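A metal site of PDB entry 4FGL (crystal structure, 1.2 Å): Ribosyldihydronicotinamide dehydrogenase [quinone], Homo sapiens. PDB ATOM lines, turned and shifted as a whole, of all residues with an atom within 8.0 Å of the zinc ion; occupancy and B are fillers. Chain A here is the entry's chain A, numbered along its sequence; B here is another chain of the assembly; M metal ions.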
ATOM      1  N   TYR A 135      23.787  23.209   5.929  1.00  0.00           N
ATOM      2  CA  TYR A 135      22.913  24.377   6.042  1.00  0.00           C
ATOM      3  C   TYR A 135      21.969  24.413   4.845  1.00  0.00           C
ATOM      4  O   TYR A 135      21.336  23.398   4.597  1.00  0.00           O
ATOM      5  CB  TYR A 135      23.703  25.677   6.324  1.00  0.00           C
ATOM      6  CG  TYR A 135      24.221  25.666   7.750  1.00  0.00           C
ATOM      7  CD1 TYR A 135      23.357  25.547   8.840  1.00  0.00           C
ATOM      8  CD2 TYR A 135      25.580  25.748   8.022  1.00  0.00           C
ATOM      9  CE1 TYR A 135      23.830  25.495  10.135  1.00  0.00           C
ATOM     10  CE2 TYR A 135      26.065  25.714   9.318  1.00  0.00           C
ATOM     11  CZ  TYR A 135      25.166  25.582  10.371  1.00  0.00           C
ATOM     12  OH  TYR A 135      25.598  25.540  11.668  1.00  0.00           O
ATOM     13  N   ASP A 136      21.858  25.521   4.122  1.00  0.00           N
ATOM     14  CA  ASP A 136      20.837  25.574   3.063  1.00  0.00           C
ATOM     15  C   ASP A 136      21.078  24.536   1.970  1.00  0.00           C
ATOM     16  O   ASP A 136      20.151  24.175   1.236  1.00  0.00           O
ATOM     17  CB  ASP A 136      20.749  26.944   2.412  1.00  0.00           C
ATOM     18  CG  ASP A 136      19.951  27.939   3.207  1.00  0.00           C
ATOM     19  OD1 ASP A 136      19.694  27.718   4.400  1.00  0.00           O
ATOM     20  OD2 ASP A 136      19.571  28.988   2.621  1.00  0.00           O
ATOM     21  N   TRP A 172      18.382  26.758  19.667  1.00  0.00           N
ATOM     22  CA  TRP A 172      19.468  26.923  18.715  1.00  0.00           C
ATOM     23  C   TRP A 172      20.190  25.613  18.305  1.00  0.00           C
ATOM     24  O   TRP A 172      20.349  25.357  17.123  1.00  0.00           O
ATOM     25  CB  TRP A 172      20.436  27.960  19.278  1.00  0.00           C
ATOM     26  CG  TRP A 172      21.687  28.189  18.517  1.00  0.00           C
ATOM     27  CD1 TRP A 172      22.930  27.803  18.852  1.00  0.00           C
ATOM     28  CD2 TRP A 172      21.819  28.932  17.298  1.00  0.00           C
ATOM     29  NE1 TRP A 172      23.834  28.233  17.937  1.00  0.00           N
ATOM     30  CE2 TRP A 172      23.179  28.946  16.960  1.00  0.00           C
ATOM     31  CE3 TRP A 172      20.914  29.605  16.466  1.00  0.00           C
ATOM     32  CZ2 TRP A 172      23.671  29.592  15.827  1.00  0.00           C
ATOM     33  CZ3 TRP A 172      21.402  30.233  15.339  1.00  0.00           C
ATOM     34  CH2 TRP A 172      22.770  30.236  15.040  1.00  0.00           C
ATOM     35  N   LEU A 174      19.088  22.632  18.276  1.00  0.00           N
ATOM     36  CA  LEU A 174      18.122  21.789  17.577  1.00  0.00           C
ATOM     37  C   LEU A 174      17.743  22.370  16.228  1.00  0.00           C
ATOM     38  O   LEU A 174      17.859  21.718  15.191  1.00  0.00           O
ATOM     39  CB  LEU A 174      16.881  21.602  18.451  1.00  0.00           C
ATOM     40  CG  LEU A 174      17.158  20.927  19.802  1.00  0.00           C
ATOM     41  CD1 LEU A 174      15.912  20.970  20.657  1.00  0.00           C
ATOM     42  CD2 LEU A 174      17.620  19.511  19.630  1.00  0.00           C
ATOM     43  N   GLN A 175      17.265  23.606  16.223  1.00  0.00           N
ATOM     44  CA  GLN A 175      16.783  24.221  14.979  1.00  0.00           C
ATOM     45  C   GLN A 175      17.938  24.553  14.031  1.00  0.00           C
ATOM     46  O   GLN A 175      17.873  24.241  12.855  1.00  0.00           O
ATOM     47  CB  GLN A 175      15.951  25.466  15.273  1.00  0.00           C
ATOM     48  CG  GLN A 175      14.640  25.088  15.957  1.00  0.00           C
ATOM     49  CD  GLN A 175      13.618  26.204  16.109  1.00  0.00           C
ATOM     50  OE1 GLN A 175      12.425  25.936  16.224  1.00  0.00           O
ATOM     51  NE2 GLN A 175      14.059  27.441  16.141  1.00  0.00           N
ATOM     52  N   HIS A 176      18.981  25.182  14.536  1.00  0.00           N
ATOM     53  CA  HIS A 176      20.077  25.585  13.672  1.00  0.00           C
ATOM     54  C   HIS A 176      21.135  24.494  13.523  1.00  0.00           C
ATOM     55  O   HIS A 176      21.503  24.094  12.407  1.00  0.00           O
ATOM     56  CB  HIS A 176      20.714  26.867  14.170  1.00  0.00           C
ATOM     57  CG  HIS A 176      21.737  27.434  13.232  1.00  0.00           C
ATOM     58  ND1 HIS A 176      21.389  28.074  12.062  1.00  0.00           N
ATOM     59  CD2 HIS A 176      23.087  27.434  13.298  1.00  0.00           C
ATOM     60  CE1 HIS A 176      22.500  28.453  11.446  1.00  0.00           C
ATOM     61  NE2 HIS A 176      23.536  28.108  12.185  1.00  0.00           N
ATOM     62  N   GLY A 177      21.656  24.038  14.651  1.00  0.00           N
ATOM     63  CA  GLY A 177      22.783  23.126  14.613  1.00  0.00           C
ATOM     64  C   GLY A 177      22.448  21.753  14.038  1.00  0.00           C
ATOM     65  O   GLY A 177      23.345  21.070  13.566  1.00  0.00           O
ATOM     66  N   THR A 178      21.178  21.357  14.094  1.00  0.00           N
ATOM     67  CA  THR A 178      20.748  20.055  13.613  1.00  0.00           C
ATOM     68  C   THR A 178      19.860  20.185  12.376  1.00  0.00           C
ATOM     69  O   THR A 178      20.224  19.761  11.283  1.00  0.00           O
ATOM     70  CB  THR A 178      20.029  19.250  14.729  1.00  0.00           C
ATOM     71  OG1 THR A 178      20.846  19.262  15.920  1.00  0.00           O
ATOM     72  CG2 THR A 178      19.797  17.818  14.313  1.00  0.00           C
ATOM     73  N   LEU A 179      18.685  20.779  12.530  1.00  0.00           N
ATOM     74  CA  LEU A 179      17.722  20.770  11.451  1.00  0.00           C
ATOM     75  C   LEU A 179      18.172  21.620  10.252  1.00  0.00           C
ATOM     76  O   LEU A 179      18.238  21.114   9.129  1.00  0.00           O
ATOM     77  CB  LEU A 179      16.354  21.202  11.983  1.00  0.00           C
ATOM     78  CG  LEU A 179      15.749  20.281  13.044  1.00  0.00           C
ATOM     79  CD1 LEU A 179      14.466  20.881  13.593  1.00  0.00           C
ATOM     80  CD2 LEU A 179      15.499  18.890  12.507  1.00  0.00           C
ATOM     81  N   HIS A 180      18.463  22.886  10.479  1.00  0.00           N
ATOM     82  CA  HIS A 180      18.958  23.718   9.397  1.00  0.00           C
ATOM     83  C   HIS A 180      20.252  23.145   8.803  1.00  0.00           C
ATOM     84  O   HIS A 180      20.448  23.146   7.582  1.00  0.00           O
ATOM     85  CB  HIS A 180      19.204  25.116   9.955  1.00  0.00           C
ATOM     86  CG  HIS A 180      19.577  26.154   8.934  1.00  0.00           C
ATOM     87  ND1 HIS A 180      19.799  27.468   9.303  1.00  0.00           N
ATOM     88  CD2 HIS A 180      19.709  26.100   7.589  1.00  0.00           C
ATOM     89  CE1 HIS A 180      20.081  28.165   8.219  1.00  0.00           C
ATOM     90  NE2 HIS A 180      20.030  27.365   7.169  1.00  0.00           N
ATOM     91  N   PHE A 181      21.133  22.644   9.656  1.00  0.00           N
ATOM     92  CA  PHE A 181      22.399  22.078   9.173  1.00  0.00           C
ATOM     93  C   PHE A 181      22.136  20.994   8.124  1.00  0.00           C
ATOM     94  O   PHE A 181      22.884  20.875   7.152  1.00  0.00           O
ATOM     95  CB  PHE A 181      23.217  21.489  10.324  1.00  0.00           C
ATOM     96  CG  PHE A 181      24.590  21.050   9.912  1.00  0.00           C
ATOM     97  CD1 PHE A 181      25.658  21.935   9.907  1.00  0.00           C
ATOM     98  CD2 PHE A 181      24.835  19.739   9.574  1.00  0.00           C
ATOM     99  CE1 PHE A 181      26.928  21.510   9.540  1.00  0.00           C
ATOM    100  CE2 PHE A 181      26.091  19.344   9.223  1.00  0.00           C
ATOM    101  CZ  PHE A 181      27.126  20.213   9.212  1.00  0.00           C
ATOM    102  N   PHE A 184      16.862  21.243   6.414  1.00  0.00           N
ATOM    103  CA  PHE A 184      15.440  21.450   6.661  1.00  0.00           C
ATOM    104  C   PHE A 184      15.118  22.943   6.662  1.00  0.00           C
ATOM    105  O   PHE A 184      15.933  23.763   7.104  1.00  0.00           O
ATOM    106  CB  PHE A 184      15.021  20.902   8.031  1.00  0.00           C
ATOM    107  CG  PHE A 184      14.919  19.407   8.133  1.00  0.00           C
ATOM    108  CD1 PHE A 184      13.758  18.748   7.725  1.00  0.00           C
ATOM    109  CD2 PHE A 184      15.940  18.677   8.686  1.00  0.00           C
ATOM    110  CE1 PHE A 184      13.645  17.379   7.882  1.00  0.00           C
ATOM    111  CE2 PHE A 184      15.829  17.317   8.841  1.00  0.00           C
ATOM    112  CZ  PHE A 184      14.676  16.664   8.423  1.00  0.00           C
ATOM    113  N   VAL A 186      12.568  25.234   8.792  1.00  0.00           N
ATOM    114  CA  VAL A 186      12.095  25.078  10.148  1.00  0.00           C
ATOM    115  C   VAL A 186      10.839  25.906  10.342  1.00  0.00           C
ATOM    116  O   VAL A 186      10.853  27.131  10.200  1.00  0.00           O
ATOM    117  CB  VAL A 186      13.178  25.483  11.176  1.00  0.00           C
ATOM    118  CG1 VAL A 186      12.651  25.333  12.581  1.00  0.00           C
ATOM    119  CG2 VAL A 186      14.420  24.626  10.984  1.00  0.00           C
ATOM    120  N   ILE A 223      10.645  29.861   9.577  1.00  0.00           N
ATOM    121  CA  ILE A 223      11.366  30.943  10.216  1.00  0.00           C
ATOM    122  C   ILE A 223      12.671  31.217   9.466  1.00  0.00           C
ATOM    123  O   ILE A 223      13.186  30.358   8.771  1.00  0.00           O
ATOM    124  CB  ILE A 223      11.688  30.615  11.687  1.00  0.00           C
ATOM    125  CG1 ILE A 223      12.731  29.492  11.808  1.00  0.00           C
ATOM    126  CG2 ILE A 223      10.412  30.249  12.438  1.00  0.00           C
ATOM    127  CD1 ILE A 223      13.219  29.262  13.231  1.00  0.00           C
ATOM    128  N   PRO A 224      13.228  32.419   9.641  1.00  0.00           N
ATOM    129  CA  PRO A 224      14.621  32.672   9.271  1.00  0.00           C
ATOM    130  C   PRO A 224      15.458  32.052  10.369  1.00  0.00           C
ATOM    131  O   PRO A 224      15.463  32.551  11.486  1.00  0.00           O
ATOM    132  CB  PRO A 224      14.707  34.200   9.264  1.00  0.00           C
ATOM    133  CG  PRO A 224      13.666  34.650  10.232  1.00  0.00           C
ATOM    134  CD  PRO A 224      12.588  33.602  10.254  1.00  0.00           C
ATOM    135  N   CYS A 225      16.099  30.925  10.081  1.00  0.00           N
ATOM    136  CA  CYS A 225      16.800  30.177  11.113  1.00  0.00           C
ATOM    137  C   CYS A 225      18.198  30.754  11.287  1.00  0.00           C
ATOM    138  O   CYS A 225      19.201  30.165  10.887  1.00  0.00           O
ATOM    139  CB  CYS A 225      16.799  28.681  10.797  1.00  0.00           C
ATOM    140  SG  CYS A 225      17.594  27.711  12.117  1.00  0.00           S
ATOM    141  N   THR A 226      18.213  31.936  11.880  1.00  0.00           N
ATOM    142  CA  THR A 226      19.427  32.723  12.047  1.00  0.00           C
ATOM    143  C   THR A 226      19.683  32.974  13.513  1.00  0.00           C
ATOM    144  O   THR A 226      18.811  32.842  14.379  1.00  0.00           O
ATOM    145  CB  THR A 226      19.247  34.083  11.366  1.00  0.00           C
ATOM    146  OG1 THR A 226      18.157  34.771  11.993  1.00  0.00           O
ATOM    147  CG2 THR A 226      18.971  33.935   9.874  1.00  0.00           C
ATOM    148  N   ALA A 227      20.905  33.393  13.811  1.00  0.00           N
ATOM    149  CA  ALA A 227      21.235  33.828  15.165  1.00  0.00           C
ATOM    150  C   ALA A 227      20.317  34.948  15.615  1.00  0.00           C
ATOM    151  O   ALA A 227      19.862  34.979  16.754  1.00  0.00           O
ATOM    152  CB  ALA A 227      22.692  34.272  15.258  1.00  0.00           C
ATOM    153  N   TRP A 229      17.167  35.532  14.826  1.00  0.00           N
ATOM    154  CA  TRP A 229      15.860  35.056  15.227  1.00  0.00           C
ATOM    155  C   TRP A 229      15.948  34.491  16.629  1.00  0.00           C
ATOM    156  O   TRP A 229      15.055  34.680  17.445  1.00  0.00           O
ATOM    157  CB  TRP A 229      15.353  33.967  14.268  1.00  0.00           C
ATOM    158  CG  TRP A 229      13.957  33.509  14.556  1.00  0.00           C
ATOM    159  CD1 TRP A 229      12.805  33.993  14.013  1.00  0.00           C
ATOM    160  CD2 TRP A 229      13.562  32.442  15.432  1.00  0.00           C
ATOM    161  NE1 TRP A 229      11.727  33.323  14.506  1.00  0.00           N
ATOM    162  CE2 TRP A 229      12.158  32.364  15.386  1.00  0.00           C
ATOM    163  CE3 TRP A 229      14.260  31.570  16.270  1.00  0.00           C
ATOM    164  CZ2 TRP A 229      11.436  31.421  16.119  1.00  0.00           C
ATOM    165  CZ3 TRP A 229      13.547  30.638  17.006  1.00  0.00           C
ATOM    166  CH2 TRP A 229      12.138  30.575  16.934  1.00  0.00           C
ATOM    167  N   HIS A 230      17.031  33.774  16.920  1.00  0.00           N
ATOM    168  CA  HIS A 230      17.129  33.070  18.189  1.00  0.00           C
ATOM    169  C   HIS A 230      17.524  33.978  19.352  1.00  0.00           C
ATOM    170  O   HIS A 230      17.057  33.774  20.485  1.00  0.00           O
ATOM    171  CB  HIS A 230      18.124  31.916  18.102  1.00  0.00           C
ATOM    172  CG  HIS A 230      17.636  30.752  17.295  1.00  0.00           C
ATOM    173  ND1 HIS A 230      17.754  30.672  15.922  1.00  0.00           N
ATOM    174  CD2 HIS A 230      17.067  29.585  17.680  1.00  0.00           C
ATOM    175  CE1 HIS A 230      17.254  29.522  15.503  1.00  0.00           C
ATOM    176  NE2 HIS A 230      16.837  28.842  16.548  1.00  0.00           N
ATOM    177  N   VAL B 163      29.381  30.335   9.984  1.00  0.00           N
ATOM    178  CA  VAL B 163      28.145  29.646   9.667  1.00  0.00           C
ATOM    179  C   VAL B 163      27.480  29.013  10.898  1.00  0.00           C
ATOM    180  O   VAL B 163      26.276  28.782  10.915  1.00  0.00           O
ATOM    181  CB  VAL B 163      28.332  28.567   8.577  1.00  0.00           C
ATOM    182  CG1 VAL B 163      28.655  29.222   7.241  1.00  0.00           C
ATOM    183  CG2 VAL B 163      29.429  27.580   8.971  1.00  0.00           C
HETATM  184 ZN    ZN M   1      19.587  28.195  11.188  1.00  0.00          ZN
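The zinc ion is bound by ND1 of His 176 (2.0 Å), O of Cys 225 (2.0 Å), ND1 of His 180 (2.0 Å) and SG of Cys 225 (2.3 Å). The zinc ion has four donor atoms within binding distance.
Within 4 Å of the zinc ion: His 176, His 180 and Cys 225. The nearest printed residue that does not touch the zinc ion is Thr 226 (4.04 Å).
A ring nitrogen (NE2) of His 176 is in hydrogen-bond range of the side-chain hydroxyl of Tyr 135 (3.3 Å). The backbone carbonyl oxygen of His 176 is in hydrogen-bond range of the backbone NH of Phe 181, 3.1 Å away. A ring nitrogen (NE2) of His 176 is in hydrogen-bond range of the backbone carbonyl oxygen (O) of Val 163 of chain B (3.1 Å). The side-chain sulfur (SG) of Cys 225 sits close to the backbone carbonyl oxygen (O) of Gln 175 (3.6 Å). The backbone NH (N) of His 180 lies within hydrogen-bond range of the backbone carbonyl oxygen (O) of Gln 175 (2.8 Å). A ring nitrogen (NE2) of His 180 lies within hydrogen-bond range of the side-chain carboxylate (OD1) of Asp 136, 2.8 Å away.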
